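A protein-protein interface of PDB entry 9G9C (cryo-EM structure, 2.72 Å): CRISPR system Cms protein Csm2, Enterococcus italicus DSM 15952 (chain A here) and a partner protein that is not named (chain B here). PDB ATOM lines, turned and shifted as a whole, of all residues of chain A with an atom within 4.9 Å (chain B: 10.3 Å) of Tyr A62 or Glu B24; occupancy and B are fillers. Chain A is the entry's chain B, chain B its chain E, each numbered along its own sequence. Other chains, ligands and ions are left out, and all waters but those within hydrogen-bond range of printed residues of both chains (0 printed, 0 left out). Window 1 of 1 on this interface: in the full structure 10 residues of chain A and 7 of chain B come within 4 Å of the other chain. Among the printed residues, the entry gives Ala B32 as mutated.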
ATOM      1  N   TYR A  58      -5.415  -8.469 -20.496  1.00  0.00           N
ATOM      2  CA  TYR A  58      -4.304  -9.442 -20.667  1.00  0.00           C
ATOM      3  C   TYR A  58      -4.670 -10.794 -20.110  1.00  0.00           C
ATOM      4  O   TYR A  58      -4.363 -11.796 -20.773  1.00  0.00           O
ATOM      5  CB  TYR A  58      -3.072  -8.858 -19.971  1.00  0.00           C
ATOM      6  CG  TYR A  58      -1.929  -9.821 -19.680  1.00  0.00           C
ATOM      7  CD1 TYR A  58      -0.943 -10.071 -20.625  1.00  0.00           C
ATOM      8  CD2 TYR A  58      -1.823 -10.452 -18.447  1.00  0.00           C
ATOM      9  CE1 TYR A  58       0.104 -10.936 -20.358  1.00  0.00           C
ATOM     10  CE2 TYR A  58      -0.782 -11.322 -18.170  1.00  0.00           C
ATOM     11  CZ  TYR A  58       0.186 -11.562 -19.128  1.00  0.00           C
ATOM     12  OH  TYR A  58       1.214 -12.415 -18.855  1.00  0.00           O
ATOM     13  N   THR A  59      -5.319 -10.843 -18.948  1.00  0.00           N
ATOM     14  CA  THR A  59      -5.559 -12.181 -18.374  1.00  0.00           C
ATOM     15  C   THR A  59      -6.450 -12.960 -19.315  1.00  0.00           C
ATOM     16  O   THR A  59      -6.153 -14.150 -19.533  1.00  0.00           O
ATOM     17  CB  THR A  59      -6.125 -12.099 -16.956  1.00  0.00           C
ATOM     18  OG1 THR A  59      -6.346 -13.458 -16.594  1.00  0.00           O
ATOM     19  CG2 THR A  59      -7.426 -11.324 -16.860  1.00  0.00           C
ATOM     20  N   LYS A  60      -7.434 -12.311 -19.935  1.00  0.00           N
ATOM     21  CA  LYS A  60      -8.286 -13.002 -20.933  1.00  0.00           C
ATOM     22  C   LYS A  60      -7.417 -13.564 -22.063  1.00  0.00           C
ATOM     23  O   LYS A  60      -7.343 -14.805 -22.194  1.00  0.00           O
ATOM     24  CB  LYS A  60      -9.277 -12.034 -21.582  1.00  0.00           C
ATOM     25  CG  LYS A  60     -10.011 -11.102 -20.641  1.00  0.00           C
ATOM     26  CD  LYS A  60     -10.831 -10.070 -21.406  1.00  0.00           C
ATOM     27  CE  LYS A  60     -11.537  -9.145 -20.474  1.00  0.00           C
ATOM     28  NZ  LYS A  60     -12.285  -9.901 -19.468  1.00  0.00           N
ATOM     29  N   VAL A  61      -6.773 -12.692 -22.841  1.00  0.00           N
ATOM     30  CA  VAL A  61      -6.019 -13.170 -24.037  1.00  0.00           C
ATOM     31  C   VAL A  61      -4.871 -14.101 -23.628  1.00  0.00           C
ATOM     32  O   VAL A  61      -4.682 -15.126 -24.314  1.00  0.00           O
ATOM     33  CB  VAL A  61      -5.470 -11.971 -24.827  1.00  0.00           C
ATOM     34  CG1 VAL A  61      -5.057 -12.365 -26.238  1.00  0.00           C
ATOM     35  CG2 VAL A  61      -6.462 -10.820 -24.865  1.00  0.00           C
ATOM     36  N   TYR A  62      -4.142 -13.779 -22.559  1.00  0.00           N
ATOM     37  CA  TYR A  62      -2.953 -14.610 -22.241  1.00  0.00           C
ATOM     38  C   TYR A  62      -3.395 -16.024 -21.929  1.00  0.00           C
ATOM     39  O   TYR A  62      -2.757 -16.980 -22.418  1.00  0.00           O
ATOM     40  CB  TYR A  62      -2.220 -14.015 -21.038  1.00  0.00           C
ATOM     41  CG  TYR A  62      -0.888 -14.684 -20.739  1.00  0.00           C
ATOM     42  CD1 TYR A  62       0.249 -14.357 -21.466  1.00  0.00           C
ATOM     43  CD2 TYR A  62      -0.765 -15.624 -19.724  1.00  0.00           C
ATOM     44  CE1 TYR A  62       1.468 -14.955 -21.203  1.00  0.00           C
ATOM     45  CE2 TYR A  62       0.449 -16.230 -19.451  1.00  0.00           C
ATOM     46  CZ  TYR A  62       1.567 -15.893 -20.192  1.00  0.00           C
ATOM     47  OH  TYR A  62       2.770 -16.479 -19.933  1.00  0.00           O
ATOM     48  N   ASN A  63      -4.471 -16.161 -21.156  1.00  0.00           N
ATOM     49  CA  ASN A  63      -5.028 -17.508 -20.862  1.00  0.00           C
ATOM     50  C   ASN A  63      -5.545 -18.162 -22.145  1.00  0.00           C
ATOM     51  O   ASN A  63      -5.346 -19.386 -22.296  1.00  0.00           O
ATOM     52  CB  ASN A  63      -6.096 -17.447 -19.775  1.00  0.00           C
ATOM     53  CG  ASN A  63      -5.491 -17.218 -18.411  1.00  0.00           C
ATOM     54  OD1 ASN A  63      -4.653 -18.008 -17.963  1.00  0.00           O
ATOM     55  ND2 ASN A  63      -5.889 -16.146 -17.743  1.00  0.00           N
ATOM     56  N   SER A  64      -6.151 -17.369 -23.036  1.00  0.00           N
ATOM     57  CA  SER A  64      -6.805 -17.921 -24.254  1.00  0.00           C
ATOM     58  C   SER A  64      -5.821 -18.660 -25.162  1.00  0.00           C
ATOM     59  O   SER A  64      -4.768 -18.082 -25.488  1.00  0.00           O
ATOM     60  CB  SER A  64      -7.508 -16.835 -25.020  1.00  0.00           C
ATOM     61  OG  SER A  64      -6.604 -16.135 -25.863  1.00  0.00           O
ATOM     62  N   LYS A 116      -2.929 -12.358 -31.043  1.00  0.00           N
ATOM     63  CA  LYS A 116      -2.541 -12.471 -29.616  1.00  0.00           C
ATOM     64  C   LYS A 116      -1.108 -11.949 -29.451  1.00  0.00           C
ATOM     65  O   LYS A 116      -0.838 -11.263 -28.445  1.00  0.00           O
ATOM     66  CB  LYS A 116      -2.564 -13.917 -29.115  1.00  0.00           C
ATOM     67  CG  LYS A 116      -2.177 -14.061 -27.650  1.00  0.00           C
ATOM     68  CD  LYS A 116      -1.736 -15.456 -27.228  1.00  0.00           C
ATOM     69  CE  LYS A 116      -2.800 -16.464 -27.490  1.00  0.00           C
ATOM     70  NZ  LYS A 116      -4.070 -16.042 -26.895  1.00  0.00           N
ATOM     71  N   LEU A 120       0.150  -9.348 -26.843  1.00  0.00           N
ATOM     72  CA  LEU A 120       1.173  -9.651 -25.816  1.00  0.00           C
ATOM     73  C   LEU A 120       2.314  -8.635 -25.961  1.00  0.00           C
ATOM     74  O   LEU A 120       2.814  -8.164 -24.923  1.00  0.00           O
ATOM     75  CB  LEU A 120       1.637 -11.094 -25.979  1.00  0.00           C
ATOM     76  CG  LEU A 120       1.116 -12.072 -24.921  1.00  0.00           C
ATOM     77  CD1 LEU A 120       1.678 -11.668 -23.571  1.00  0.00           C
ATOM     78  CD2 LEU A 120      -0.402 -12.078 -24.881  1.00  0.00           C
ATOM     79  N   GLY B  20       0.250 -24.466  -6.689  1.00  0.00           N
ATOM     80  CA  GLY B  20       1.140 -23.626  -7.465  1.00  0.00           C
ATOM     81  C   GLY B  20       1.976 -24.408  -8.459  1.00  0.00           C
ATOM     82  O   GLY B  20       2.298 -25.579  -8.264  1.00  0.00           O
ATOM     83  N   GLY B  21       2.315 -23.740  -9.557  1.00  0.00           N
ATOM     84  CA  GLY B  21       3.268 -24.260 -10.516  1.00  0.00           C
ATOM     85  C   GLY B  21       4.147 -23.156 -11.064  1.00  0.00           C
ATOM     86  O   GLY B  21       3.644 -22.196 -11.656  1.00  0.00           O
ATOM     87  N   GLY B  22       5.455 -23.302 -10.878  1.00  0.00           N
ATOM     88  CA  GLY B  22       6.348 -22.217 -11.309  1.00  0.00           C
ATOM     89  C   GLY B  22       6.997 -22.484 -12.643  1.00  0.00           C
ATOM     90  O   GLY B  22       6.447 -23.286 -13.423  1.00  0.00           O
ATOM     91  N   GLY B  23       8.101 -21.787 -12.933  1.00  0.00           N
ATOM     92  CA  GLY B  23       8.847 -22.012 -14.187  1.00  0.00           C
ATOM     93  C   GLY B  23       8.637 -20.894 -15.188  1.00  0.00           C
ATOM     94  O   GLY B  23       9.381 -20.853 -16.186  1.00  0.00           O
ATOM     95  N   GLU B  24       7.653 -20.027 -14.946  1.00  0.00           N
ATOM     96  CA  GLU B  24       7.333 -18.945 -15.908  1.00  0.00           C
ATOM     97  C   GLU B  24       7.523 -17.581 -15.237  1.00  0.00           C
ATOM     98  O   GLU B  24       6.987 -17.395 -14.123  1.00  0.00           O
ATOM     99  CB  GLU B  24       5.884 -19.132 -16.350  1.00  0.00           C
ATOM    100  CG  GLU B  24       5.430 -18.141 -17.416  1.00  0.00           C
ATOM    101  CD  GLU B  24       3.923 -18.174 -17.587  1.00  0.00           C
ATOM    102  OE1 GLU B  24       3.212 -17.834 -16.618  1.00  0.00           O
ATOM    103  OE2 GLU B  24       3.460 -18.559 -18.681  1.00  0.00           O
ATOM    104  N   THR B  25       8.257 -16.666 -15.879  1.00  0.00           N
ATOM    105  CA  THR B  25       8.383 -15.299 -15.326  1.00  0.00           C
ATOM    106  C   THR B  25       7.022 -14.639 -15.397  1.00  0.00           C
ATOM    107  O   THR B  25       6.315 -14.860 -16.404  1.00  0.00           O
ATOM    108  CB  THR B  25       9.451 -14.506 -16.077  1.00  0.00           C
ATOM    109  OG1 THR B  25      10.604 -15.341 -16.119  1.00  0.00           O
ATOM    110  CG2 THR B  25       9.793 -13.206 -15.372  1.00  0.00           C
ATOM    111  N   SER B  26       6.660 -13.848 -14.384  1.00  0.00           N
ATOM    112  CA  SER B  26       5.298 -13.255 -14.351  1.00  0.00           C
ATOM    113  C   SER B  26       5.339 -11.770 -14.731  1.00  0.00           C
ATOM    114  O   SER B  26       6.306 -11.084 -14.341  1.00  0.00           O
ATOM    115  CB  SER B  26       4.652 -13.453 -13.008  1.00  0.00           C
ATOM    116  OG  SER B  26       3.378 -12.825 -12.976  1.00  0.00           O
ATOM    117  N   MET B  27       4.320 -11.300 -15.453  1.00  0.00           N
ATOM    118  CA  MET B  27       4.250  -9.899 -15.839  1.00  0.00           C
ATOM    119  C   MET B  27       4.005  -9.021 -14.616  1.00  0.00           C
ATOM    120  O   MET B  27       3.345  -9.427 -13.656  1.00  0.00           O
ATOM    121  CB  MET B  27       3.147  -9.702 -16.887  1.00  0.00           C
ATOM    122  CG  MET B  27       2.552  -8.308 -16.966  1.00  0.00           C
ATOM    123  SD  MET B  27       1.975  -7.913 -18.628  1.00  0.00           S
ATOM    124  CE  MET B  27       0.498  -6.974 -18.260  1.00  0.00           C
ATOM    125  N   ILE B  28       4.585  -7.816 -14.661  1.00  0.00           N
ATOM    126  CA  ILE B  28       4.428  -6.844 -13.542  1.00  0.00           C
ATOM    127  C   ILE B  28       2.945  -6.495 -13.392  1.00  0.00           C
ATOM    128  O   ILE B  28       2.309  -6.145 -14.407  1.00  0.00           O
ATOM    129  CB  ILE B  28       5.298  -5.596 -13.780  1.00  0.00           C
ATOM    130  CG1 ILE B  28       6.779  -5.953 -13.753  1.00  0.00           C
ATOM    131  CG2 ILE B  28       4.968  -4.488 -12.782  1.00  0.00           C
ATOM    132  CD1 ILE B  28       7.671  -4.928 -14.425  1.00  0.00           C
ATOM    133  N   ALA B  30       0.596  -8.581 -12.678  1.00  0.00           N
ATOM    134  CA  ALA B  30      -0.212  -9.765 -12.908  1.00  0.00           C
ATOM    135  C   ALA B  30      -0.113 -10.687 -11.695  1.00  0.00           C
ATOM    136  O   ALA B  30       0.383 -10.302 -10.633  1.00  0.00           O
ATOM    137  CB  ALA B  30       0.225 -10.459 -14.195  1.00  0.00           C
ATOM    138  N   ILE B  31      -0.590 -11.919 -11.841  1.00  0.00           N
ATOM    139  CA  ILE B  31      -0.538 -12.884 -10.749  1.00  0.00           C
ATOM    140  C   ILE B  31       0.908 -13.310 -10.532  1.00  0.00           C
ATOM    141  O   ILE B  31       1.583 -13.764 -11.463  1.00  0.00           O
ATOM    142  CB  ILE B  31      -1.438 -14.089 -11.041  1.00  0.00           C
ATOM    143  CG1 ILE B  31      -2.894 -13.637 -11.167  1.00  0.00           C
ATOM    144  CG2 ILE B  31      -1.284 -15.141  -9.962  1.00  0.00           C
ATOM    145  CD1 ILE B  31      -3.739 -14.529 -12.042  1.00  0.00           C
ATOM    146  N   ALA B  32       1.392 -13.156  -9.298  1.00  0.00           N
ATOM    147  CA  ALA B  32       2.761 -13.558  -8.991  1.00  0.00           C
ATOM    148  C   ALA B  32       2.897 -15.075  -8.943  1.00  0.00           C
ATOM    149  O   ALA B  32       3.853 -15.635  -9.491  1.00  0.00           O
ATOM    150  CB  ALA B  32       3.204 -12.935  -7.667  1.00  0.00           C
ATOM    151  N   SER B  33       1.952 -15.754  -8.299  1.00  0.00           N
ATOM    152  CA  SER B  33       1.986 -17.210  -8.152  1.00  0.00           C
ATOM    153  C   SER B  33       0.789 -17.831  -8.857  1.00  0.00           C
ATOM    154  O   SER B  33      -0.326 -17.837  -8.307  1.00  0.00           O
ATOM    155  CB  SER B  33       1.999 -17.602  -6.675  1.00  0.00           C
ATOM    156  OG  SER B  33       3.031 -16.929  -5.975  1.00  0.00           O
ATOM    157  N   PRO B  34       0.960 -18.357 -10.065  1.00  0.00           N
ATOM    158  CA  PRO B  34      -0.149 -19.020 -10.756  1.00  0.00           C
ATOM    159  C   PRO B  34      -0.342 -20.448 -10.263  1.00  0.00           C
ATOM    160  O   PRO B  34       0.444 -20.986  -9.483  1.00  0.00           O
ATOM    161  CB  PRO B  34       0.292 -18.995 -12.222  1.00  0.00           C
ATOM    162  CG  PRO B  34       1.776 -19.002 -12.154  1.00  0.00           C
ATOM    163  CD  PRO B  34       2.150 -18.225 -10.922  1.00  0.00           C
ATOM    164  N   VAL B  35      -1.422 -21.062 -10.739  1.00  0.00           N
ATOM    165  CA  VAL B  35      -1.743 -22.449 -10.425  1.00  0.00           C
ATOM    166  C   VAL B  35      -1.170 -23.341 -11.514  1.00  0.00           C
ATOM    167  O   VAL B  35      -0.977 -22.916 -12.659  1.00  0.00           O
ATOM    168  CB  VAL B  35      -3.264 -22.669 -10.285  1.00  0.00           C
ATOM    169  CG1 VAL B  35      -3.799 -21.937  -9.075  1.00  0.00           C
ATOM    170  CG2 VAL B  35      -3.985 -22.231 -11.548  1.00  0.00           C
ATOM    171  N   VAL B  36      -0.916 -24.601 -11.152  1.00  0.00           N
ATOM    172  CA  VAL B  36      -0.446 -25.586 -12.169  1.00  0.00           C
ATOM    173  C   VAL B  36      -1.609 -25.831 -13.141  1.00  0.00           C
ATOM    174  O   VAL B  36      -2.745 -26.053 -12.675  1.00  0.00           O
ATOM    175  CB  VAL B  36       0.055 -26.901 -11.538  1.00  0.00           C
ATOM    176  CG1 VAL B  36      -0.945 -27.504 -10.561  1.00  0.00           C
ATOM    177  CG2 VAL B  36       0.473 -27.923 -12.587  1.00  0.00           C
ATOM    178  N   ARG B  37      -1.339 -25.754 -14.439  1.00  0.00           N
ATOM    179  CA  ARG B  37      -2.395 -25.957 -15.457  1.00  0.00           C
ATOM    180  C   ARG B  37      -1.891 -26.998 -16.459  1.00  0.00           C
ATOM    181  O   ARG B  37      -0.673 -27.015 -16.711  1.00  0.00           O
ATOM    182  CB  ARG B  37      -2.702 -24.619 -16.140  1.00  0.00           C
ATOM    183  CG  ARG B  37      -3.155 -23.542 -15.166  1.00  0.00           C
ATOM    184  CD  ARG B  37      -3.385 -22.193 -15.818  1.00  0.00           C
ATOM    185  NE  ARG B  37      -4.624 -22.178 -16.600  1.00  0.00           N
ATOM    186  CZ  ARG B  37      -5.645 -21.367 -16.368  1.00  0.00           C
ATOM    187  NH1 ARG B  37      -5.516 -20.379 -15.504  1.00  0.00           N
ATOM    188  NH2 ARG B  37      -6.788 -21.543 -17.005  1.00  0.00           N
ATOM    189  N   PRO B  39      -0.671 -28.145 -19.826  1.00  0.00           N
ATOM    190  CA  PRO B  39      -0.189 -27.289 -20.899  1.00  0.00           C
ATOM    191  C   PRO B  39      -1.064 -27.308 -22.135  1.00  0.00           C
ATOM    192  O   PRO B  39      -1.303 -26.240 -22.723  1.00  0.00           O
ATOM    193  CB  PRO B  39       1.204 -27.879 -21.159  1.00  0.00           C
ATOM    194  CG  PRO B  39       1.564 -28.554 -19.861  1.00  0.00           C
ATOM    195  CD  PRO B  39       0.258 -29.191 -19.446  1.00  0.00           C
ATOM    196  N   SER B  41      -4.416 -28.188 -22.604  1.00  0.00           N
ATOM    197  CA  SER B  41      -5.760 -27.582 -22.416  1.00  0.00           C
ATOM    198  C   SER B  41      -5.664 -26.208 -21.745  1.00  0.00           C
ATOM    199  O   SER B  41      -6.676 -25.490 -21.771  1.00  0.00           O
ATOM    200  CB  SER B  41      -6.656 -28.492 -21.627  1.00  0.00           C
ATOM    201  OG  SER B  41      -6.191 -28.625 -20.293  1.00  0.00           O
ATOM    202  N   ARG B  42      -4.492 -25.840 -21.226  1.00  0.00           N
ATOM    203  CA  ARG B  42      -4.342 -24.564 -20.474  1.00  0.00           C
ATOM    204  C   ARG B  42      -5.326 -24.569 -19.293  1.00  0.00           C
ATOM    205  O   ARG B  42      -5.465 -23.514 -18.647  1.00  0.00           O
ATOM    206  CB  ARG B  42      -4.493 -23.365 -21.417  1.00  0.00           C
ATOM    207  CG  ARG B  42      -3.695 -23.504 -22.706  1.00  0.00           C
ATOM    208  CD  ARG B  42      -3.489 -22.166 -23.387  1.00  0.00           C
ATOM    209  NE  ARG B  42      -2.635 -21.288 -22.582  1.00  0.00           N
ATOM    210  CZ  ARG B  42      -2.284 -20.057 -22.926  1.00  0.00           C
ATOM    211  NH1 ARG B  42      -2.795 -19.502 -24.009  1.00  0.00           N
ATOM    212  NH2 ARG B  42      -1.431 -19.381 -22.178  1.00  0.00           N
ATOM    213  N   LEU B  43      -5.964 -25.708 -19.028  1.00  0.00           N
ATOM    214  CA  LEU B  43      -6.944 -25.808 -17.916  1.00  0.00           C
ATOM    215  C   LEU B  43      -6.203 -26.249 -16.654  1.00  0.00           C
ATOM    216  O   LEU B  43      -5.317 -27.114 -16.762  1.00  0.00           O
ATOM    217  CB  LEU B  43      -8.059 -26.794 -18.261  1.00  0.00           C
ATOM    218  CG  LEU B  43      -9.396 -26.203 -18.716  1.00  0.00           C
ATOM    219  CD1 LEU B  43      -9.242 -25.379 -19.975  1.00  0.00           C
ATOM    220  CD2 LEU B  43     -10.377 -27.331 -18.957  1.00  0.00           C
ATOM    221  N   THR B 119     -10.281 -19.800 -13.397  1.00  0.00           N
ATOM    222  CA  THR B 119      -9.469 -19.354 -12.276  1.00  0.00           C
ATOM    223  C   THR B 119      -9.801 -17.911 -11.925  1.00  0.00           C
ATOM    224  O   THR B 119     -10.154 -17.108 -12.794  1.00  0.00           O
ATOM    225  CB  THR B 119      -7.973 -19.487 -12.579  1.00  0.00           C
ATOM    226  OG1 THR B 119      -7.664 -18.791 -13.792  1.00  0.00           O
ATOM    227  CG2 THR B 119      -7.578 -20.952 -12.709  1.00  0.00           C
ATOM    228  N   GLU B 140      -3.495 -16.754  -8.043  1.00  0.00           N
ATOM    229  CA  GLU B 140      -4.505 -17.452  -8.822  1.00  0.00           C
ATOM    230  C   GLU B 140      -5.090 -18.607  -8.017  1.00  0.00           C
ATOM    231  O   GLU B 140      -4.371 -19.317  -7.308  1.00  0.00           O
ATOM    232  CB  GLU B 140      -3.894 -17.960 -10.126  1.00  0.00           C
ATOM    233  CG  GLU B 140      -4.880 -18.128 -11.258  1.00  0.00           C
ATOM    234  CD  GLU B 140      -4.231 -18.676 -12.512  1.00  0.00           C
ATOM    235  OE1 GLU B 140      -3.026 -18.998 -12.469  1.00  0.00           O
ATOM    236  OE2 GLU B 140      -4.922 -18.780 -13.544  1.00  0.00           O
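The side-chain amide nitrogen (ND2) of Asn A63 is in hydrogen-bond range of the backbone carbonyl oxygen (O) of Thr A59 (2.7 Å). The side-chain hydroxyl (OG) of Ser A64 lies within hydrogen-bond range of the backbone carbonyl oxygen (O) of Val A61 (2.7 Å). O of Ser A64 is in hydrogen-bond range of NZ of Lys A116 (2.6 Å). The guanidinium group (NE) of Arg B37 lies within hydrogen-bond range of the backbone carbonyl oxygen (O) of Arg B42 (2.6 Å). NH1 of Arg B37 lies within hydrogen-bond range of OG1 of Thr B119 (3.2 Å). NH1 of Arg B37 is in salt-bridge range of OE2 of Glu B140 (2.6 Å).
Of the 9 printed residues of chain A, 4 touch a printed residue of chain B. Printed residues of chain A that touch a printed residue of chain B: Tyr A58, Tyr A62, Asn A63 and Ser A64. Of the 23 printed residues of chain B, 4 touch a printed residue of chain A. Hydrophobic or aromatic side chains of chain B within 4 Å of the printed part of chain A: Met B27. Among the printed residues, no Asp or Glu carboxylate lies within 4 Å of a Lys or Arg side-chain nitrogen of the other chain.
Printed residues of chain B within 4 Å of Tyr A58: Met B27. No residue of chain B comes within 4 Å of Val A61. Of the printed residues of chain B, Tyr A62 touches Glu B24 and Arg B42. Of chain A, only Tyr A62 comes within 4 Å of Glu B24. Thr B25 touches none of the printed residues of chain A. Of the printed residues of chain A, Met B27 touches Tyr A58. Val B36 touches none of the printed residues of chain A. Printed residues of chain A within 4 Å of Arg B37: Asn A63. Of the printed residues of chain A, Arg B42 touches Tyr A62 (2.8 Å), Asn A63 (3.1 Å) and Ser A64 (2.8 Å).
The side-chain carboxylate of Glu B24 lies within hydrogen-bond range of the side-chain hydroxyl of Tyr A62, at 2.5 Å. The backbone carbonyl oxygen (O) of Tyr A62 lies within hydrogen-bond range of the guanidinium group (NH2) of Arg B42, at 2.8 Å. O of Asn A63 is in hydrogen-bond range of NH1 of Arg B42 (3.1 Å). The backbone carbonyl oxygen (O) of Ser A64 lies within hydrogen-bond range of the guanidinium group (NH1) of Arg B42, 2.8 Å away.
Among the printed residues, merely in contact across the chains: Asn A63 with Arg B37 (3.5 Å) and Tyr A58 with Met B27 (3.9 Å).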
